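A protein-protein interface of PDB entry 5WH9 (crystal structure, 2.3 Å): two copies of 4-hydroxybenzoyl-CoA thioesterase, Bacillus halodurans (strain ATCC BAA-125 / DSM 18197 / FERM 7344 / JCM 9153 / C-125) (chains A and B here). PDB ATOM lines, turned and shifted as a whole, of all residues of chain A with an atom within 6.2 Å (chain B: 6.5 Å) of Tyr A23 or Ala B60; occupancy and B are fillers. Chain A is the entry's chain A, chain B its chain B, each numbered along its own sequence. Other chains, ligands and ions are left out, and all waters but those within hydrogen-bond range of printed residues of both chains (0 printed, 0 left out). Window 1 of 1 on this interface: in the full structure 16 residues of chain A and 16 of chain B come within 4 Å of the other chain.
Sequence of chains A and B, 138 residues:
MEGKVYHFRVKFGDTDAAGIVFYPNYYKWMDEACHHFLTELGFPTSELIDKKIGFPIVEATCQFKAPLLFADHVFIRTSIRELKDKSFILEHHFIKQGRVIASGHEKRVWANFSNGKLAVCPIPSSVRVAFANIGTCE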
ATOM      1  N   ASP A  14      16.386   1.558  13.835  1.00  0.00           N
ATOM      2  CA  ASP A  14      17.297   0.568  14.399  1.00  0.00           C
ATOM      3  C   ASP A  14      16.974  -0.824  13.913  1.00  0.00           C
ATOM      4  O   ASP A  14      17.789  -1.743  14.067  1.00  0.00           O
ATOM      5  CB  ASP A  14      17.244   0.597  15.926  1.00  0.00           C
ATOM      6  CG  ASP A  14      17.722   1.904  16.494  1.00  0.00           C
ATOM      7  OD1 ASP A  14      18.607   2.521  15.856  1.00  0.00           O
ATOM      8  OD2 ASP A  14      17.208   2.315  17.566  1.00  0.00           O
ATOM      9  N   ASP A  16      15.650  -3.764  10.998  1.00  0.00           N
ATOM     10  CA  ASP A  16      15.913  -4.085   9.599  1.00  0.00           C
ATOM     11  C   ASP A  16      14.719  -4.829   9.016  1.00  0.00           C
ATOM     12  O   ASP A  16      13.660  -4.911   9.644  1.00  0.00           O
ATOM     13  CB  ASP A  16      17.205  -4.883   9.457  1.00  0.00           C
ATOM     14  CG  ASP A  16      17.178  -6.181  10.237  1.00  0.00           C
ATOM     15  OD1 ASP A  16      16.176  -6.923  10.109  1.00  0.00           O
ATOM     16  OD2 ASP A  16      18.158  -6.450  10.970  1.00  0.00           O
ATOM     17  N   VAL A  21      15.820  -5.848  15.601  1.00  0.00           N
ATOM     18  CA  VAL A  21      17.016  -5.006  15.547  1.00  0.00           C
ATOM     19  C   VAL A  21      18.160  -5.590  14.703  1.00  0.00           C
ATOM     20  O   VAL A  21      18.451  -6.784  14.773  1.00  0.00           O
ATOM     21  CB  VAL A  21      17.548  -4.697  16.959  1.00  0.00           C
ATOM     22  CG1 VAL A  21      18.790  -3.824  16.879  1.00  0.00           C
ATOM     23  CG2 VAL A  21      16.470  -4.026  17.797  1.00  0.00           C
ATOM     24  N   PHE A  22      18.790  -4.709  13.928  1.00  0.00           N
ATOM     25  CA  PHE A  22      20.000  -4.969  13.157  1.00  0.00           C
ATOM     26  C   PHE A  22      21.101  -5.001  14.173  1.00  0.00           C
ATOM     27  O   PHE A  22      21.323  -4.044  14.828  1.00  0.00           O
ATOM     28  CB  PHE A  22      20.199  -3.824  12.172  1.00  0.00           C
ATOM     29  CG  PHE A  22      21.433  -3.895  11.330  1.00  0.00           C
ATOM     30  CD1 PHE A  22      21.690  -4.960  10.546  1.00  0.00           C
ATOM     31  CD2 PHE A  22      22.325  -2.855  11.309  1.00  0.00           C
ATOM     32  CE1 PHE A  22      22.821  -4.994   9.750  1.00  0.00           C
ATOM     33  CE2 PHE A  22      23.446  -2.879  10.525  1.00  0.00           C
ATOM     34  CZ  PHE A  22      23.696  -3.958   9.743  1.00  0.00           C
ATOM     35  N   TYR A  23      21.793  -6.113  14.272  1.00  0.00           N
ATOM     36  CA  TYR A  23      22.569  -6.428  15.441  1.00  0.00           C
ATOM     37  C   TYR A  23      23.685  -5.473  15.791  1.00  0.00           C
ATOM     38  O   TYR A  23      23.913  -5.236  16.926  1.00  0.00           O
ATOM     39  CB  TYR A  23      23.069  -7.884  15.463  1.00  0.00           C
ATOM     40  CG  TYR A  23      24.434  -8.124  14.914  1.00  0.00           C
ATOM     41  CD1 TYR A  23      25.536  -7.920  15.657  1.00  0.00           C
ATOM     42  CD2 TYR A  23      24.589  -8.545  13.666  1.00  0.00           C
ATOM     43  CE1 TYR A  23      26.769  -8.117  15.159  1.00  0.00           C
ATOM     44  CE2 TYR A  23      25.801  -8.791  13.136  1.00  0.00           C
ATOM     45  CZ  TYR A  23      26.903  -8.573  13.887  1.00  0.00           C
ATOM     46  OH  TYR A  23      28.097  -8.818  13.341  1.00  0.00           O
ATOM     47  N   PRO A  24      24.394  -4.955  14.794  1.00  0.00           N
ATOM     48  CA  PRO A  24      25.431  -3.998  15.130  1.00  0.00           C
ATOM     49  C   PRO A  24      24.998  -2.833  16.017  1.00  0.00           C
ATOM     50  O   PRO A  24      25.859  -2.265  16.582  1.00  0.00           O
ATOM     51  CB  PRO A  24      25.897  -3.466  13.767  1.00  0.00           C
ATOM     52  CG  PRO A  24      25.681  -4.517  12.849  1.00  0.00           C
ATOM     53  CD  PRO A  24      24.414  -5.090  13.258  1.00  0.00           C
ATOM     54  N   ASN A  25      23.718  -2.492  16.037  1.00  0.00           N
ATOM     55  CA  ASN A  25      23.189  -1.467  16.918  1.00  0.00           C
ATOM     56  C   ASN A  25      23.429  -1.793  18.393  1.00  0.00           C
ATOM     57  O   ASN A  25      23.546  -0.887  19.222  1.00  0.00           O
ATOM     58  CB  ASN A  25      21.694  -1.235  16.650  1.00  0.00           C
ATOM     59  CG  ASN A  25      21.440  -0.483  15.349  1.00  0.00           C
ATOM     60  OD1 ASN A  25      20.618  -0.883  14.542  1.00  0.00           O
ATOM     61  ND2 ASN A  25      22.140   0.612  15.156  1.00  0.00           N
ATOM     62  N   TYR A  26      23.496  -3.081  18.733  1.00  0.00           N
ATOM     63  CA  TYR A  26      23.814  -3.453  20.123  1.00  0.00           C
ATOM     64  C   TYR A  26      25.151  -2.907  20.575  1.00  0.00           C
ATOM     65  O   TYR A  26      25.330  -2.640  21.752  1.00  0.00           O
ATOM     66  CB  TYR A  26      23.811  -4.959  20.321  1.00  0.00           C
ATOM     67  CG  TYR A  26      22.443  -5.589  20.245  1.00  0.00           C
ATOM     68  CD1 TYR A  26      21.842  -5.819  19.026  1.00  0.00           C
ATOM     69  CD2 TYR A  26      21.763  -5.972  21.400  1.00  0.00           C
ATOM     70  CE1 TYR A  26      20.595  -6.407  18.948  1.00  0.00           C
ATOM     71  CE2 TYR A  26      20.535  -6.570  21.335  1.00  0.00           C
ATOM     72  CZ  TYR A  26      19.950  -6.786  20.104  1.00  0.00           C
ATOM     73  OH  TYR A  26      18.718  -7.385  20.017  1.00  0.00           O
ATOM     74  N   TYR A  27      26.093  -2.736  19.647  1.00  0.00           N
ATOM     75  CA  TYR A  27      27.404  -2.146  19.989  1.00  0.00           C
ATOM     76  C   TYR A  27      27.334  -0.623  20.084  1.00  0.00           C
ATOM     77  O   TYR A  27      28.103   0.015  20.792  1.00  0.00           O
ATOM     78  CB  TYR A  27      28.473  -2.583  18.983  1.00  0.00           C
ATOM     79  CG  TYR A  27      28.594  -4.075  18.948  1.00  0.00           C
ATOM     80  CD1 TYR A  27      27.746  -4.833  18.161  1.00  0.00           C
ATOM     81  CD2 TYR A  27      29.514  -4.736  19.751  1.00  0.00           C
ATOM     82  CE1 TYR A  27      27.822  -6.202  18.150  1.00  0.00           C
ATOM     83  CE2 TYR A  27      29.593  -6.111  19.758  1.00  0.00           C
ATOM     84  CZ  TYR A  27      28.751  -6.838  18.948  1.00  0.00           C
ATOM     85  OH  TYR A  27      28.809  -8.214  18.939  1.00  0.00           O
ATOM     86  N   ALA A  60      35.457  -6.038  21.576  1.00  0.00           N
ATOM     87  CA  ALA A  60      34.076  -6.045  21.976  1.00  0.00           C
ATOM     88  C   ALA A  60      33.451  -7.364  21.645  1.00  0.00           C
ATOM     89  O   ALA A  60      33.798  -7.993  20.704  1.00  0.00           O
ATOM     90  CB  ALA A  60      33.310  -4.905  21.335  1.00  0.00           C
ATOM     91  N   THR A  61      32.491  -7.753  22.437  1.00  0.00           N
ATOM     92  CA  THR A  61      31.767  -8.999  22.236  1.00  0.00           C
ATOM     93  C   THR A  61      30.345  -8.832  22.731  1.00  0.00           C
ATOM     94  O   THR A  61      30.089  -8.060  23.653  1.00  0.00           O
ATOM     95  CB  THR A  61      32.398 -10.160  23.027  1.00  0.00           C
ATOM     96  OG1 THR A  61      33.822 -10.098  22.916  1.00  0.00           O
ATOM     97  CG2 THR A  61      31.911 -11.496  22.498  1.00  0.00           C
ATOM     98  N   CYS A  62      29.423  -9.571  22.131  1.00  0.00           N
ATOM     99  CA  CYS A  62      28.047  -9.534  22.578  1.00  0.00           C
ATOM    100  C   CYS A  62      27.379 -10.828  22.198  1.00  0.00           C
ATOM    101  O   CYS A  62      27.636 -11.377  21.123  1.00  0.00           O
ATOM    102  CB  CYS A  62      27.301  -8.343  21.963  1.00  0.00           C
ATOM    103  SG  CYS A  62      25.724  -7.951  22.757  1.00  0.00           S
ATOM    104  N   GLN A  63      26.536 -11.319  23.100  1.00  0.00           N
ATOM    105  CA  GLN A  63      25.778 -12.538  22.891  1.00  0.00           C
ATOM    106  C   GLN A  63      24.300 -12.201  23.001  1.00  0.00           C
ATOM    107  O   GLN A  63      23.891 -11.477  23.915  1.00  0.00           O
ATOM    108  CB  GLN A  63      26.167 -13.563  23.942  1.00  0.00           C
ATOM    109  CG  GLN A  63      25.391 -14.841  23.843  1.00  0.00           C
ATOM    110  CD  GLN A  63      25.716 -15.786  24.962  1.00  0.00           C
ATOM    111  OE1 GLN A  63      25.375 -15.531  26.124  1.00  0.00           O
ATOM    112  NE2 GLN A  63      26.393 -16.889  24.627  1.00  0.00           N
ATOM    113  N   PHE A  64      23.508 -12.712  22.068  1.00  0.00           N
ATOM    114  CA  PHE A  64      22.130 -12.274  21.893  1.00  0.00           C
ATOM    115  C   PHE A  64      21.126 -13.377  22.232  1.00  0.00           C
ATOM    116  O   PHE A  64      21.072 -14.403  21.550  1.00  0.00           O
ATOM    117  CB  PHE A  64      21.936 -11.829  20.442  1.00  0.00           C
ATOM    118  CG  PHE A  64      22.963 -10.826  19.972  1.00  0.00           C
ATOM    119  CD1 PHE A  64      24.149 -11.248  19.393  1.00  0.00           C
ATOM    120  CD2 PHE A  64      22.743  -9.461  20.114  1.00  0.00           C
ATOM    121  CE1 PHE A  64      25.090 -10.333  18.954  1.00  0.00           C
ATOM    122  CE2 PHE A  64      23.687  -8.538  19.676  1.00  0.00           C
ATOM    123  CZ  PHE A  64      24.860  -8.973  19.099  1.00  0.00           C
ATOM    124  N   TYR B  26      32.382  -1.940  12.362  1.00  0.00           N
ATOM    125  CA  TYR B  26      33.069  -3.178  12.018  1.00  0.00           C
ATOM    126  C   TYR B  26      32.071  -4.349  11.975  1.00  0.00           C
ATOM    127  O   TYR B  26      32.235  -5.295  11.202  1.00  0.00           O
ATOM    128  CB  TYR B  26      34.185  -3.481  13.015  1.00  0.00           C
ATOM    129  CG  TYR B  26      35.388  -2.579  12.927  1.00  0.00           C
ATOM    130  CD1 TYR B  26      35.361  -1.311  13.470  1.00  0.00           C
ATOM    131  CD2 TYR B  26      36.572  -3.013  12.333  1.00  0.00           C
ATOM    132  CE1 TYR B  26      36.456  -0.479  13.407  1.00  0.00           C
ATOM    133  CE2 TYR B  26      37.687  -2.191  12.268  1.00  0.00           C
ATOM    134  CZ  TYR B  26      37.617  -0.914  12.809  1.00  0.00           C
ATOM    135  OH  TYR B  26      38.713  -0.062  12.775  1.00  0.00           O
ATOM    136  N   TYR B  27      31.044  -4.290  12.819  1.00  0.00           N
ATOM    137  CA  TYR B  27      30.017  -5.336  12.849  1.00  0.00           C
ATOM    138  C   TYR B  27      29.087  -5.226  11.651  1.00  0.00           C
ATOM    139  O   TYR B  27      28.676  -6.242  11.096  1.00  0.00           O
ATOM    140  CB  TYR B  27      29.248  -5.297  14.179  1.00  0.00           C
ATOM    141  CG  TYR B  27      30.188  -5.494  15.348  1.00  0.00           C
ATOM    142  CD1 TYR B  27      30.519  -6.774  15.779  1.00  0.00           C
ATOM    143  CD2 TYR B  27      30.798  -4.411  15.981  1.00  0.00           C
ATOM    144  CE1 TYR B  27      31.400  -6.981  16.830  1.00  0.00           C
ATOM    145  CE2 TYR B  27      31.716  -4.609  17.039  1.00  0.00           C
ATOM    146  CZ  TYR B  27      32.000  -5.909  17.448  1.00  0.00           C
ATOM    147  OH  TYR B  27      32.864  -6.151  18.503  1.00  0.00           O
ATOM    148  N   LYS B  28      28.779  -3.990  11.255  1.00  0.00           N
ATOM    149  CA  LYS B  28      28.023  -3.697  10.044  1.00  0.00           C
ATOM    150  C   LYS B  28      28.760  -4.312   8.854  1.00  0.00           C
ATOM    151  O   LYS B  28      28.162  -4.971   7.996  1.00  0.00           O
ATOM    152  CB  LYS B  28      27.885  -2.162   9.899  1.00  0.00           C
ATOM    153  CG  LYS B  28      27.388  -1.581   8.566  1.00  0.00           C
ATOM    154  CD  LYS B  28      27.960  -0.141   8.376  1.00  0.00           C
ATOM    155  CE  LYS B  28      27.210   0.739   7.352  1.00  0.00           C
ATOM    156  NZ  LYS B  28      27.254   0.338   5.883  1.00  0.00           N
ATOM    157  N   MET B  30      30.994  -6.761   8.882  1.00  0.00           N
ATOM    158  CA  MET B  30      30.932  -8.220   8.964  1.00  0.00           C
ATOM    159  C   MET B  30      29.574  -8.721   8.527  1.00  0.00           C
ATOM    160  O   MET B  30      29.462  -9.708   7.792  1.00  0.00           O
ATOM    161  CB  MET B  30      31.223  -8.725  10.370  1.00  0.00           C
ATOM    162  CG  MET B  30      32.693  -8.694  10.709  1.00  0.00           C
ATOM    163  SD  MET B  30      33.070  -9.422  12.317  1.00  0.00           S
ATOM    164  CE  MET B  30      31.974  -8.480  13.376  1.00  0.00           C
ATOM    165  N   ASP B  31      28.529  -8.037   8.956  1.00  0.00           N
ATOM    166  CA  ASP B  31      27.214  -8.424   8.482  1.00  0.00           C
ATOM    167  C   ASP B  31      27.189  -8.377   6.943  1.00  0.00           C
ATOM    168  O   ASP B  31      26.671  -9.290   6.291  1.00  0.00           O
ATOM    169  CB  ASP B  31      26.140  -7.529   9.080  1.00  0.00           C
ATOM    170  CG  ASP B  31      24.757  -7.998   8.740  1.00  0.00           C
ATOM    171  OD1 ASP B  31      24.232  -8.883   9.439  1.00  0.00           O
ATOM    172  OD2 ASP B  31      24.190  -7.487   7.764  1.00  0.00           O
ATOM    173  N   ILE B  57      22.307 -13.726  14.076  1.00  0.00           N
ATOM    174  CA  ILE B  57      23.512 -13.797  14.872  1.00  0.00           C
ATOM    175  C   ILE B  57      23.149 -14.305  16.267  1.00  0.00           C
ATOM    176  O   ILE B  57      22.109 -13.931  16.817  1.00  0.00           O
ATOM    177  CB  ILE B  57      24.134 -12.402  14.979  1.00  0.00           C
ATOM    178  CG1 ILE B  57      25.558 -12.476  15.507  1.00  0.00           C
ATOM    179  CG2 ILE B  57      23.267 -11.486  15.859  1.00  0.00           C
ATOM    180  CD1 ILE B  57      26.538 -12.839  14.445  1.00  0.00           C
ATOM    181  N   VAL B  58      23.983 -15.165  16.845  1.00  0.00           N
ATOM    182  CA  VAL B  58      23.814 -15.501  18.265  1.00  0.00           C
ATOM    183  C   VAL B  58      24.926 -14.895  19.114  1.00  0.00           C
ATOM    184  O   VAL B  58      24.750 -14.656  20.315  1.00  0.00           O
ATOM    185  CB  VAL B  58      23.745 -17.010  18.520  1.00  0.00           C
ATOM    186  CG1 VAL B  58      22.398 -17.549  18.125  1.00  0.00           C
ATOM    187  CG2 VAL B  58      24.788 -17.707  17.742  1.00  0.00           C
ATOM    188  N   GLU B  59      26.065 -14.638  18.477  1.00  0.00           N
ATOM    189  CA  GLU B  59      27.222 -14.091  19.163  1.00  0.00           C
ATOM    190  C   GLU B  59      28.191 -13.450  18.163  1.00  0.00           C
ATOM    191  O   GLU B  59      28.351 -13.939  17.059  1.00  0.00           O
ATOM    192  CB  GLU B  59      27.913 -15.205  19.954  1.00  0.00           C
ATOM    193  CG  GLU B  59      29.095 -14.757  20.796  1.00  0.00           C
ATOM    194  CD  GLU B  59      29.509 -15.813  21.809  1.00  0.00           C
ATOM    195  OE1 GLU B  59      29.169 -17.008  21.607  1.00  0.00           O
ATOM    196  OE2 GLU B  59      30.154 -15.445  22.820  1.00  0.00           O
ATOM    197  N   ALA B  60      28.830 -12.349  18.547  1.00  0.00           N
ATOM    198  CA  ALA B  60      29.796 -11.711  17.658  1.00  0.00           C
ATOM    199  C   ALA B  60      30.918 -11.010  18.414  1.00  0.00           C
ATOM    200  O   ALA B  60      30.686 -10.361  19.431  1.00  0.00           O
ATOM    201  CB  ALA B  60      29.098 -10.749  16.696  1.00  0.00           C
ATOM    202  N   THR B  61      32.135 -11.139  17.895  1.00  0.00           N
ATOM    203  CA  THR B  61      33.330 -10.660  18.570  1.00  0.00           C
ATOM    204  C   THR B  61      34.260  -9.990  17.574  1.00  0.00           C
ATOM    205  O   THR B  61      34.431 -10.460  16.459  1.00  0.00           O
ATOM    206  CB  THR B  61      34.099 -11.818  19.207  1.00  0.00           C
ATOM    207  OG1 THR B  61      33.183 -12.717  19.839  1.00  0.00           O
ATOM    208  CG2 THR B  61      35.087 -11.298  20.241  1.00  0.00           C
ATOM    209  N   CYS B  62      34.873  -8.892  17.972  1.00  0.00           N
ATOM    210  CA  CYS B  62      35.837  -8.260  17.107  1.00  0.00           C
ATOM    211  C   CYS B  62      36.990  -7.698  17.925  1.00  0.00           C
ATOM    212  O   CYS B  62      36.831  -7.236  19.069  1.00  0.00           O
ATOM    213  CB  CYS B  62      35.193  -7.176  16.216  1.00  0.00           C
ATOM    214  SG  CYS B  62      36.154  -6.821  14.653  1.00  0.00           S
ATOM    215  N   HIS B 105      34.601 -12.798  14.634  1.00  0.00           N
ATOM    216  CA  HIS B 105      33.770 -13.864  14.113  1.00  0.00           C
ATOM    217  C   HIS B 105      32.326 -13.586  14.455  1.00  0.00           C
ATOM    218  O   HIS B 105      32.020 -12.735  15.293  1.00  0.00           O
ATOM    219  CB  HIS B 105      34.209 -15.237  14.652  1.00  0.00           C
ATOM    220  CG  HIS B 105      34.054 -15.389  16.130  1.00  0.00           C
ATOM    221  ND1 HIS B 105      32.879 -15.812  16.718  1.00  0.00           N
ATOM    222  CD2 HIS B 105      34.927 -15.174  17.144  1.00  0.00           C
ATOM    223  CE1 HIS B 105      33.033 -15.845  18.030  1.00  0.00           C
ATOM    224  NE2 HIS B 105      34.267 -15.465  18.314  1.00  0.00           N
ATOM    225  N   GLU B 106      31.444 -14.301  13.782  1.00  0.00           N
ATOM    226  CA  GLU B 106      30.034 -14.286  14.077  1.00  0.00           C
ATOM    227  C   GLU B 106      29.625 -15.745  14.291  1.00  0.00           C
ATOM    228  O   GLU B 106      29.949 -16.608  13.477  1.00  0.00           O
ATOM    229  CB  GLU B 106      29.266 -13.713  12.879  1.00  0.00           C
ATOM    230  CG  GLU B 106      29.611 -12.270  12.507  1.00  0.00           C
ATOM    231  CD  GLU B 106      28.854 -11.773  11.283  1.00  0.00           C
ATOM    232  OE1 GLU B 106      28.423 -10.602  11.292  1.00  0.00           O
ATOM    233  OE2 GLU B 106      28.708 -12.536  10.297  1.00  0.00           O
ATOM    234  N   LYS B 107      28.945 -16.034  15.391  1.00  0.00           N
ATOM    235  CA  LYS B 107      28.210 -17.284  15.490  1.00  0.00           C
ATOM    236  C   LYS B 107      26.798 -17.047  14.981  1.00  0.00           C
ATOM    237  O   LYS B 107      26.107 -16.142  15.451  1.00  0.00           O
ATOM    238  CB  LYS B 107      28.144 -17.775  16.929  1.00  0.00           C
ATOM    239  CG  LYS B 107      27.488 -19.149  17.063  1.00  0.00           C
ATOM    240  CD  LYS B 107      27.909 -19.867  18.352  1.00  0.00           C
ATOM    241  CE  LYS B 107      27.162 -21.189  18.481  1.00  0.00           C
ATOM    242  NZ  LYS B 107      27.639 -22.039  19.623  1.00  0.00           N
ATOM    243  N   ARG B 108      26.369 -17.842  14.009  1.00  0.00           N
ATOM    244  CA  ARG B 108      25.028 -17.682  13.458  1.00  0.00           C
ATOM    245  C   ARG B 108      24.258 -19.001  13.412  1.00  0.00           C
ATOM    246  O   ARG B 108      24.840 -20.087  13.347  1.00  0.00           O
ATOM    247  CB  ARG B 108      25.079 -17.053  12.061  1.00  0.00           C
ATOM    248  CG  ARG B 108      25.729 -15.677  11.980  1.00  0.00           C
ATOM    249  CD  ARG B 108      25.705 -15.178  10.539  1.00  0.00           C
ATOM    250  NE  ARG B 108      26.225 -13.825  10.360  1.00  0.00           N
ATOM    251  CZ  ARG B 108      25.466 -12.733  10.282  1.00  0.00           C
ATOM    252  NH1 ARG B 108      24.147 -12.832  10.380  1.00  0.00           N
ATOM    253  NH2 ARG B 108      26.026 -11.540  10.105  1.00  0.00           N
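N of Phe A22 sits at hydrogen-bond distance from O of Asp A14, 3.1 Å away.
The side-chain hydroxyl (OH) of Tyr B27 sits close to the backbone NH (N) of Cys B62, at 3.4 Å.
The backbone NH (N) of Asp B31 is in hydrogen-bond range of the side-chain carboxylate (OE1) of Glu B106, at 3.5 Å.
The backbone carbonyl oxygen (O) of Glu B59 sits at hydrogen-bond distance from the backbone NH (N) of Lys B107.
O of Thr B61 sits at hydrogen-bond distance from N of His B105.
The guanidinium group (NE) of Arg B108 is in salt-bridge range of the side-chain carboxylate (OE2) of Glu B106, 2.8 Å away.
Among the printed residues, merely in contact across the chains: Phe A22 with Asp B31, Tyr A23 with Met B30, Tyr A23 with Ile B57, Tyr A23 with Ala B60, Pro A24 with Tyr B27, Pro A24 with Lys B28, Tyr A27 with Tyr B27, Ala A60 with Thr B61, Thr A61 with Ala B60, Thr A61 with Thr B61, Cys A62 with Glu B59, Gln A63 with Val B58 and Phe A64 with Ile B57.
Tyr A27 touches its own counterpart, Tyr B27.
Ala A60 touches Thr B61, and with the chains exchanged Thr A61 touches Ala B60.
Ala A60 touches Cys B62, and with the chains exchanged Cys A62 touches Ala B60.
Thr B61 touches its own counterpart, Thr A61.
Of the 20 pairs that touch across the chains among the printed residues, 8 have their exchanged pair printed and touching as well.
Printed residues of chain B within 4 Å of Tyr A23: Tyr B27 (3.5 Å), Met B30 (3.9 Å), Ile B57 (3.6 Å), Ala B60 (3.8 Å) and Glu B106 (2.7 Å).
Of chain A, only Tyr A23, Tyr A27, Thr A61 and Cys A62 come within 4 Å of Ala B60.
Printed residues of chain A within 4 Å of Lys B28: Pro A24 (3.5 Å).
Of the printed residues of chain A, Asp B31 touches Phe A22 (3.5 Å).
Of the printed residues of chain B, Pro A24 touches Tyr B27 (3.7 Å) and Lys B28 (3.5 Å).
Asp A16 touches none of the printed residues of chain B.
The nearest printed residue of chain B that does not touch Tyr A23 is Asp B31 (4.02 Å).
Of the 14 printed residues of chain A, 9 touch a printed residue of chain B.
Printed residues of chain A that touch a printed residue of chain B: Phe A22, Tyr A23, Pro A24, Tyr A27, Ala A60, Thr A61, Cys A62, Gln A63 and Phe A64.
Hydrophobic or aromatic side chains of chain A that line the printed part of chain B: Phe A22, Tyr A23, Pro A24, Tyr A27, Ala A60 and Phe A64.
Printed residues of chain B that touch a printed residue of chain A: Tyr B27, Lys B28, Met B30, Asp B31, Ile B57, Val B58, Glu B59, Ala B60, Thr B61, Cys B62 and Glu B106.
OH of Tyr A23 lies within hydrogen-bond range of O of Tyr B27 (3.5 Å).
OH of Tyr A23 lies within hydrogen-bond range of OE1 of Glu B106 (2.7 Å).
The backbone carbonyl oxygen of Ala B60 sits at hydrogen-bond distance from the side-chain hydroxyl of Tyr A27 (2.9 Å).
The backbone carbonyl oxygen of Ala A60 lies within hydrogen-bond range of the side-chain hydroxyl of Tyr B27, at 3.0 Å.
O of Ala A60 lies within hydrogen-bond range of N of Cys B62, at 3.1 Å.
O of Cys A62 is in hydrogen-bond range of N of Ala B60, at 3.0 Å.
O of Val B58 is in hydrogen-bond range of N of Phe A64, at 2.9 Å.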
